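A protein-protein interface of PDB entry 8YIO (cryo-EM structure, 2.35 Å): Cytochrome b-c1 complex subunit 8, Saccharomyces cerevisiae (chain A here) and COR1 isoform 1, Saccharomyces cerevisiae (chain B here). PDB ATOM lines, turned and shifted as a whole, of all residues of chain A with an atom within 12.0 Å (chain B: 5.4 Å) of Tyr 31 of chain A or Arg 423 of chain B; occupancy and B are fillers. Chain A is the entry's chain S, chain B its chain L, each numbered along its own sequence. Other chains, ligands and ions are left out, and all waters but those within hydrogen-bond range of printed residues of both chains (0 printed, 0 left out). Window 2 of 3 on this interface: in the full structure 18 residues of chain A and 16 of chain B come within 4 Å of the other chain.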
ATOM      1  N   ALA A  27     -19.020 -26.309  22.319  1.00  0.00           N
ATOM      2  CA  ALA A  27     -18.383 -27.003  21.207  1.00  0.00           C
ATOM      3  C   ALA A  27     -18.422 -26.127  19.961  1.00  0.00           C
ATOM      4  O   ALA A  27     -19.280 -25.257  19.820  1.00  0.00           O
ATOM      5  CB  ALA A  27     -19.049 -28.356  20.931  1.00  0.00           C
ATOM      6  N   VAL A  28     -17.475 -26.374  19.053  1.00  0.00           N
ATOM      7  CA  VAL A  28     -17.338 -25.650  17.792  1.00  0.00           C
ATOM      8  C   VAL A  28     -17.450 -26.659  16.650  1.00  0.00           C
ATOM      9  O   VAL A  28     -17.032 -27.813  16.796  1.00  0.00           O
ATOM     10  CB  VAL A  28     -16.000 -24.866  17.746  1.00  0.00           C
ATOM     11  CG1 VAL A  28     -15.822 -24.067  16.460  1.00  0.00           C
ATOM     12  CG2 VAL A  28     -15.911 -23.907  18.911  1.00  0.00           C
ATOM     13  N   SER A  29     -18.057 -26.234  15.536  1.00  0.00           N
ATOM     14  CA  SER A  29     -18.242 -27.080  14.362  1.00  0.00           C
ATOM     15  C   SER A  29     -16.902 -27.538  13.784  1.00  0.00           C
ATOM     16  O   SER A  29     -15.942 -26.761  13.751  1.00  0.00           O
ATOM     17  CB  SER A  29     -19.019 -26.320  13.286  1.00  0.00           C
ATOM     18  OG  SER A  29     -19.143 -27.084  12.103  1.00  0.00           O
ATOM     19  N   PRO A  30     -16.805 -28.789  13.325  1.00  0.00           N
ATOM     20  CA  PRO A  30     -15.573 -29.245  12.658  1.00  0.00           C
ATOM     21  C   PRO A  30     -15.284 -28.552  11.338  1.00  0.00           C
ATOM     22  O   PRO A  30     -14.124 -28.537  10.912  1.00  0.00           O
ATOM     23  CB  PRO A  30     -15.824 -30.744  12.447  1.00  0.00           C
ATOM     24  CG  PRO A  30     -16.863 -31.099  13.443  1.00  0.00           C
ATOM     25  CD  PRO A  30     -17.735 -29.901  13.580  1.00  0.00           C
ATOM     26  N   TYR A  31     -16.293 -27.980  10.678  1.00  0.00           N
ATOM     27  CA  TYR A  31     -16.076 -27.249   9.436  1.00  0.00           C
ATOM     28  C   TYR A  31     -15.363 -25.921   9.651  1.00  0.00           C
ATOM     29  O   TYR A  31     -14.861 -25.344   8.683  1.00  0.00           O
ATOM     30  CB  TYR A  31     -17.407 -27.001   8.730  1.00  0.00           C
ATOM     31  CG  TYR A  31     -18.000 -28.226   8.086  1.00  0.00           C
ATOM     32  CD1 TYR A  31     -17.611 -28.620   6.813  1.00  0.00           C
ATOM     33  CD2 TYR A  31     -18.944 -28.993   8.753  1.00  0.00           C
ATOM     34  CE1 TYR A  31     -18.149 -29.744   6.222  1.00  0.00           C
ATOM     35  CE2 TYR A  31     -19.487 -30.116   8.174  1.00  0.00           C
ATOM     36  CZ  TYR A  31     -19.087 -30.487   6.906  1.00  0.00           C
ATOM     37  OH  TYR A  31     -19.626 -31.606   6.327  1.00  0.00           O
ATOM     38  N   ALA A  32     -15.302 -25.426  10.887  1.00  0.00           N
ATOM     39  CA  ALA A  32     -14.672 -24.151  11.196  1.00  0.00           C
ATOM     40  C   ALA A  32     -13.353 -24.313  11.942  1.00  0.00           C
ATOM     41  O   ALA A  32     -12.860 -23.348  12.531  1.00  0.00           O
ATOM     42  CB  ALA A  32     -15.628 -23.275  12.004  1.00  0.00           C
ATOM     43  N   GLN A  33     -12.766 -25.503  11.927  1.00  0.00           N
ATOM     44  CA  GLN A  33     -11.524 -25.766  12.637  1.00  0.00           C
ATOM     45  C   GLN A  33     -10.386 -26.018  11.655  1.00  0.00           C
ATOM     46  O   GLN A  33     -10.603 -26.249  10.463  1.00  0.00           O
ATOM     47  CB  GLN A  33     -11.678 -26.955  13.591  1.00  0.00           C
ATOM     48  CG  GLN A  33     -12.674 -26.712  14.713  1.00  0.00           C
ATOM     49  CD  GLN A  33     -12.684 -27.817  15.749  1.00  0.00           C
ATOM     50  OE1 GLN A  33     -11.636 -28.309  16.153  1.00  0.00           O
ATOM     51  NE2 GLN A  33     -13.872 -28.211  16.183  1.00  0.00           N
ATOM     52  N   LYS A  34      -9.163 -25.962  12.177  1.00  0.00           N
ATOM     53  CA  LYS A  34      -7.980 -26.173  11.353  1.00  0.00           C
ATOM     54  C   LYS A  34      -7.861 -27.640  10.952  1.00  0.00           C
ATOM     55  O   LYS A  34      -8.074 -28.531  11.780  1.00  0.00           O
ATOM     56  CB  LYS A  34      -6.718 -25.757  12.103  1.00  0.00           C
ATOM     57  CG  LYS A  34      -6.549 -24.268  12.287  1.00  0.00           C
ATOM     58  CD  LYS A  34      -5.239 -23.969  12.986  1.00  0.00           C
ATOM     59  CE  LYS A  34      -4.983 -22.480  13.061  1.00  0.00           C
ATOM     60  NZ  LYS A  34      -5.316 -21.942  14.409  1.00  0.00           N
ATOM     61  N   PRO A  35      -7.511 -27.926   9.698  1.00  0.00           N
ATOM     62  CA  PRO A  35      -7.382 -29.326   9.271  1.00  0.00           C
ATOM     63  C   PRO A  35      -6.048 -29.921   9.710  1.00  0.00           C
ATOM     64  O   PRO A  35      -4.985 -29.517   9.236  1.00  0.00           O
ATOM     65  CB  PRO A  35      -7.497 -29.246   7.744  1.00  0.00           C
ATOM     66  CG  PRO A  35      -7.087 -27.846   7.390  1.00  0.00           C
ATOM     67  CD  PRO A  35      -7.297 -26.971   8.594  1.00  0.00           C
ATOM     68  N   LEU A  36      -6.250 -31.079  10.791  1.00  0.00           N
ATOM     69  CA  LEU A  36      -5.019 -31.854  10.993  1.00  0.00           C
ATOM     70  C   LEU A  36      -3.877 -31.020  11.583  1.00  0.00           C
ATOM     71  O   LEU A  36      -2.922 -30.632  10.910  1.00  0.00           O
ATOM     72  CB  LEU A  36      -4.575 -32.573   9.713  1.00  0.00           C
ATOM     73  CG  LEU A  36      -5.297 -33.910   9.538  1.00  0.00           C
ATOM     74  CD1 LEU A  36      -4.634 -34.727   8.458  1.00  0.00           C
ATOM     75  CD2 LEU A  36      -5.369 -34.687  10.843  1.00  0.00           C
ATOM     76  N   ASP B 402     -26.752 -27.294   3.107  1.00  0.00           N
ATOM     77  CA  ASP B 402     -25.400 -27.686   3.534  1.00  0.00           C
ATOM     78  C   ASP B 402     -24.647 -26.546   4.228  1.00  0.00           C
ATOM     79  O   ASP B 402     -23.507 -26.233   3.891  1.00  0.00           O
ATOM     80  CB  ASP B 402     -24.590 -28.243   2.357  1.00  0.00           C
ATOM     81  CG  ASP B 402     -23.532 -29.228   2.791  1.00  0.00           C
ATOM     82  OD1 ASP B 402     -23.879 -30.235   3.438  1.00  0.00           O
ATOM     83  OD2 ASP B 402     -22.348 -28.999   2.484  1.00  0.00           O
ATOM     84  N   GLN B 403     -25.281 -25.940   5.227  1.00  0.00           N
ATOM     85  CA  GLN B 403     -24.700 -24.811   5.939  1.00  0.00           C
ATOM     86  C   GLN B 403     -24.552 -25.121   7.423  1.00  0.00           C
ATOM     87  O   GLN B 403     -25.176 -26.042   7.954  1.00  0.00           O
ATOM     88  CB  GLN B 403     -25.547 -23.543   5.752  1.00  0.00           C
ATOM     89  CG  GLN B 403     -25.629 -23.050   4.320  1.00  0.00           C
ATOM     90  CD  GLN B 403     -24.319 -22.471   3.819  1.00  0.00           C
ATOM     91  OE1 GLN B 403     -23.546 -21.904   4.582  1.00  0.00           O
ATOM     92  NE2 GLN B 403     -24.067 -22.619   2.530  1.00  0.00           N
ATOM     93  N   ASP B 404     -23.720 -24.325   8.093  1.00  0.00           N
ATOM     94  CA  ASP B 404     -23.471 -24.474   9.522  1.00  0.00           C
ATOM     95  C   ASP B 404     -24.621 -23.904  10.347  1.00  0.00           C
ATOM     96  O   ASP B 404     -25.313 -22.972   9.931  1.00  0.00           O
ATOM     97  CB  ASP B 404     -22.163 -23.782   9.907  1.00  0.00           C
ATOM     98  CG  ASP B 404     -20.980 -24.734   9.934  1.00  0.00           C
ATOM     99  OD1 ASP B 404     -21.186 -25.961   9.848  1.00  0.00           O
ATOM    100  OD2 ASP B 404     -19.837 -24.253  10.040  1.00  0.00           O
ATOM    101  N   ILE B 405     -24.814 -24.473  11.539  1.00  0.00           N
ATOM    102  CA  ILE B 405     -25.927 -24.135  12.417  1.00  0.00           C
ATOM    103  C   ILE B 405     -25.400 -23.768  13.799  1.00  0.00           C
ATOM    104  O   ILE B 405     -24.251 -24.040  14.145  1.00  0.00           O
ATOM    105  CB  ILE B 405     -26.945 -25.290  12.532  1.00  0.00           C
ATOM    106  CG1 ILE B 405     -26.238 -26.580  12.951  1.00  0.00           C
ATOM    107  CG2 ILE B 405     -27.693 -25.486  11.224  1.00  0.00           C
ATOM    108  CD1 ILE B 405     -27.163 -27.728  13.228  1.00  0.00           C
ATOM    109  N   TYR B 419     -23.554 -32.731  17.683  1.00  0.00           N
ATOM    110  CA  TYR B 419     -23.583 -31.712  16.635  1.00  0.00           C
ATOM    111  C   TYR B 419     -23.575 -32.310  15.229  1.00  0.00           C
ATOM    112  O   TYR B 419     -24.322 -31.850  14.360  1.00  0.00           O
ATOM    113  CB  TYR B 419     -22.403 -30.752  16.810  1.00  0.00           C
ATOM    114  CG  TYR B 419     -22.441 -29.552  15.889  1.00  0.00           C
ATOM    115  CD1 TYR B 419     -23.176 -28.422  16.222  1.00  0.00           C
ATOM    116  CD2 TYR B 419     -21.742 -29.549  14.685  1.00  0.00           C
ATOM    117  CE1 TYR B 419     -23.220 -27.331  15.383  1.00  0.00           C
ATOM    118  CE2 TYR B 419     -21.789 -28.470  13.839  1.00  0.00           C
ATOM    119  CZ  TYR B 419     -22.522 -27.360  14.194  1.00  0.00           C
ATOM    120  OH  TYR B 419     -22.558 -26.277  13.354  1.00  0.00           O
ATOM    121  N   MET B 420     -22.745 -33.327  14.984  1.00  0.00           N
ATOM    122  CA  MET B 420     -22.566 -33.817  13.620  1.00  0.00           C
ATOM    123  C   MET B 420     -23.752 -34.632  13.123  1.00  0.00           C
ATOM    124  O   MET B 420     -23.960 -34.720  11.908  1.00  0.00           O
ATOM    125  CB  MET B 420     -21.283 -34.642  13.515  1.00  0.00           C
ATOM    126  CG  MET B 420     -20.019 -33.802  13.457  1.00  0.00           C
ATOM    127  SD  MET B 420     -20.122 -32.425  12.294  1.00  0.00           S
ATOM    128  CE  MET B 420     -19.975 -33.270  10.734  1.00  0.00           C
ATOM    129  N   ARG B 421     -24.533 -35.231  14.025  1.00  0.00           N
ATOM    130  CA  ARG B 421     -25.767 -35.886  13.607  1.00  0.00           C
ATOM    131  C   ARG B 421     -26.816 -34.874  13.167  1.00  0.00           C
ATOM    132  O   ARG B 421     -27.618 -35.162  12.273  1.00  0.00           O
ATOM    133  CB  ARG B 421     -26.319 -36.757  14.736  1.00  0.00           C
ATOM    134  CG  ARG B 421     -25.764 -38.170  14.779  1.00  0.00           C
ATOM    135  CD  ARG B 421     -26.327 -39.040  13.662  1.00  0.00           C
ATOM    136  NE  ARG B 421     -27.721 -39.406  13.887  1.00  0.00           N
ATOM    137  CZ  ARG B 421     -28.121 -40.571  14.387  1.00  0.00           C
ATOM    138  NH1 ARG B 421     -29.413 -40.810  14.554  1.00  0.00           N
ATOM    139  NH2 ARG B 421     -27.235 -41.497  14.722  1.00  0.00           N
ATOM    140  N   ILE B 422     -26.825 -33.689  13.777  1.00  0.00           N
ATOM    141  CA  ILE B 422     -27.783 -32.650  13.411  1.00  0.00           C
ATOM    142  C   ILE B 422     -27.293 -31.865  12.198  1.00  0.00           C
ATOM    143  O   ILE B 422     -28.091 -31.442  11.355  1.00  0.00           O
ATOM    144  CB  ILE B 422     -28.043 -31.743  14.628  1.00  0.00           C
ATOM    145  CG1 ILE B 422     -28.398 -32.595  15.844  1.00  0.00           C
ATOM    146  CG2 ILE B 422     -29.160 -30.750  14.356  1.00  0.00           C
ATOM    147  CD1 ILE B 422     -28.529 -31.816  17.123  1.00  0.00           C
ATOM    148  N   ARG B 423     -25.974 -31.676  12.084  1.00  0.00           N
ATOM    149  CA  ARG B 423     -25.389 -30.948  10.961  1.00  0.00           C
ATOM    150  C   ARG B 423     -25.567 -31.697   9.644  1.00  0.00           C
ATOM    151  O   ARG B 423     -25.747 -31.072   8.595  1.00  0.00           O
ATOM    152  CB  ARG B 423     -23.909 -30.680  11.255  1.00  0.00           C
ATOM    153  CG  ARG B 423     -23.068 -30.097  10.127  1.00  0.00           C
ATOM    154  CD  ARG B 423     -23.551 -28.730   9.699  1.00  0.00           C
ATOM    155  NE  ARG B 423     -22.639 -28.089   8.757  1.00  0.00           N
ATOM    156  CZ  ARG B 423     -22.637 -28.299   7.445  1.00  0.00           C
ATOM    157  NH1 ARG B 423     -21.770 -27.661   6.676  1.00  0.00           N
ATOM    158  NH2 ARG B 423     -23.497 -29.146   6.900  1.00  0.00           N
ATOM    159  N   SER B 424     -25.572 -33.029   9.681  1.00  0.00           N
ATOM    160  CA  SER B 424     -25.721 -33.818   8.466  1.00  0.00           C
ATOM    161  C   SER B 424     -27.150 -33.844   7.941  1.00  0.00           C
ATOM    162  O   SER B 424     -27.360 -34.253   6.795  1.00  0.00           O
ATOM    163  CB  SER B 424     -25.233 -35.248   8.706  1.00  0.00           C
ATOM    164  OG  SER B 424     -26.155 -35.980   9.489  1.00  0.00           O
ATOM    165  N   ASP B 425     -28.128 -33.413   8.731  1.00  0.00           N
ATOM    166  CA  ASP B 425     -29.508 -33.325   8.275  1.00  0.00           C
ATOM    167  C   ASP B 425     -29.799 -32.050   7.493  1.00  0.00           C
ATOM    168  O   ASP B 425     -30.937 -31.862   7.057  1.00  0.00           O
ATOM    169  CB  ASP B 425     -30.463 -33.429   9.465  1.00  0.00           C
ATOM    170  CG  ASP B 425     -30.985 -34.834   9.673  1.00  0.00           C
ATOM    171  OD1 ASP B 425     -30.710 -35.708   8.827  1.00  0.00           O
ATOM    172  OD2 ASP B 425     -31.678 -35.069  10.683  1.00  0.00           O
ATOM    173  N   MET B 426     -28.813 -31.176   7.306  1.00  0.00           N
ATOM    174  CA  MET B 426     -28.992 -29.970   6.510  1.00  0.00           C
ATOM    175  C   MET B 426     -28.884 -30.228   5.013  1.00  0.00           C
ATOM    176  O   MET B 426     -29.094 -29.302   4.226  1.00  0.00           O
ATOM    177  CB  MET B 426     -27.977 -28.904   6.929  1.00  0.00           C
ATOM    178  CG  MET B 426     -28.113 -28.447   8.372  1.00  0.00           C
ATOM    179  SD  MET B 426     -29.731 -27.759   8.768  1.00  0.00           S
ATOM    180  CE  MET B 426     -29.641 -26.168   7.968  1.00  0.00           C
ATOM    181  N   SER B 427     -28.556 -31.450   4.606  1.00  0.00           N
ATOM    182  CA  SER B 427     -28.669 -31.883   3.224  1.00  0.00           C
ATOM    183  C   SER B 427     -29.364 -33.231   3.175  1.00  0.00           C
ATOM    184  O   SER B 427     -29.342 -34.003   4.136  1.00  0.00           O
ATOM    185  CB  SER B 427     -27.306 -32.009   2.527  1.00  0.00           C
ATOM    186  OG  SER B 427     -26.701 -30.752   2.332  1.00  0.00           O
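OG of Ser 29 of chain A lies within hydrogen-bond range of OD1 of Asp 404 of chain B.
The backbone carbonyl oxygen (O) of Ile 405 of chain B sits at hydrogen-bond distance from the side-chain hydroxyl (OH) of Tyr 419 of chain B (2.9 Å).
The side-chain hydroxyl (OG) of Ser 29 of chain A sits close to the backbone NH (N) of Tyr 31 of chain A (3.3 Å).
OD1 of Asp 402 of chain B is in salt-bridge range of NH2 of Arg 423 of chain B, 3.6 Å away.
The side-chain carboxylate (OD1) of Asp 404 of chain B is in salt-bridge range of the guanidinium group (NE) of Arg 423 of chain B, at 2.8 Å.
The backbone carbonyl oxygen of Gln 403 of chain B is in hydrogen-bond range of the guanidinium group of Arg 423 of chain B, at 3.4 Å.
Among the printed residues, merely in contact across the chains: Ser 29 of chain A with Tyr 419 of chain B, Pro 30 of chain A with Met 420 of chain B, Tyr 31 of chain A with Asp 404 of chain B and Tyr 31 of chain A with Arg 423 of chain B.
Of the printed residues of chain B, Tyr 31 of chain A touches Asp 404 (3.9 Å) and Arg 423 (3.7 Å).
Arg 423 of chain B touches just one residue of chain A: Tyr 31 (3.7 Å).
Asp 402 of chain B touches none of the printed residues of chain A.
No residue of chain A comes within 4 Å of Gln 403 of chain B.
Asp 404 of chain B touches two residues of chain A.
No residue of chain A comes within 4 Å of Ile 405 of chain B.
Tyr 419 of chain B touches just one residue of chain A: Ser 29 (3.5 Å).
Met 420 of chain B touches one residue of chain A.
No residue of chain A comes within 4 Å of Ser 424 of chain B.
No residue of chain A comes within 4 Å of Asp 425 of chain B.
No residue of chain A comes within 4 Å of Met 426 of chain B.
No residue of chain A comes within 4 Å of Ser 427 of chain B.
Of the printed residues of chain B, Ser 29 of chain A touches Asp 404 (3.2 Å) and Tyr 419 (3.5 Å).
Of the printed residues of chain B, Pro 30 of chain A touches Met 420 (3.7 Å).
Arg 421 of chain B touches none of the printed residues of chain A.
Leu 36 of chain A touches none of the printed residues of chain B.
The nearest residue of chain B that does not touch Tyr 31 of chain A is Met 420 of chain B (4.1 Å).
The nearest printed residue of chain B that does not touch Ser 29 of chain A is Arg 423 of chain B (4.9 Å).
Hydrophobic or aromatic side chains of chain B within 4 Å of the printed part of chain A: Tyr 419 and Met 420.
Along chain B the printed residues that touch a printed residue of chain A span positions 404 to 423.
Of the 10 printed residues of chain A, 3 touch a printed residue of chain B.
Printed residues of chain A that touch a printed residue of chain B: Ser 29, Pro 30 and Tyr 31.
Along chain A the printed residues that touch a printed residue of chain B span positions 29 to 31.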
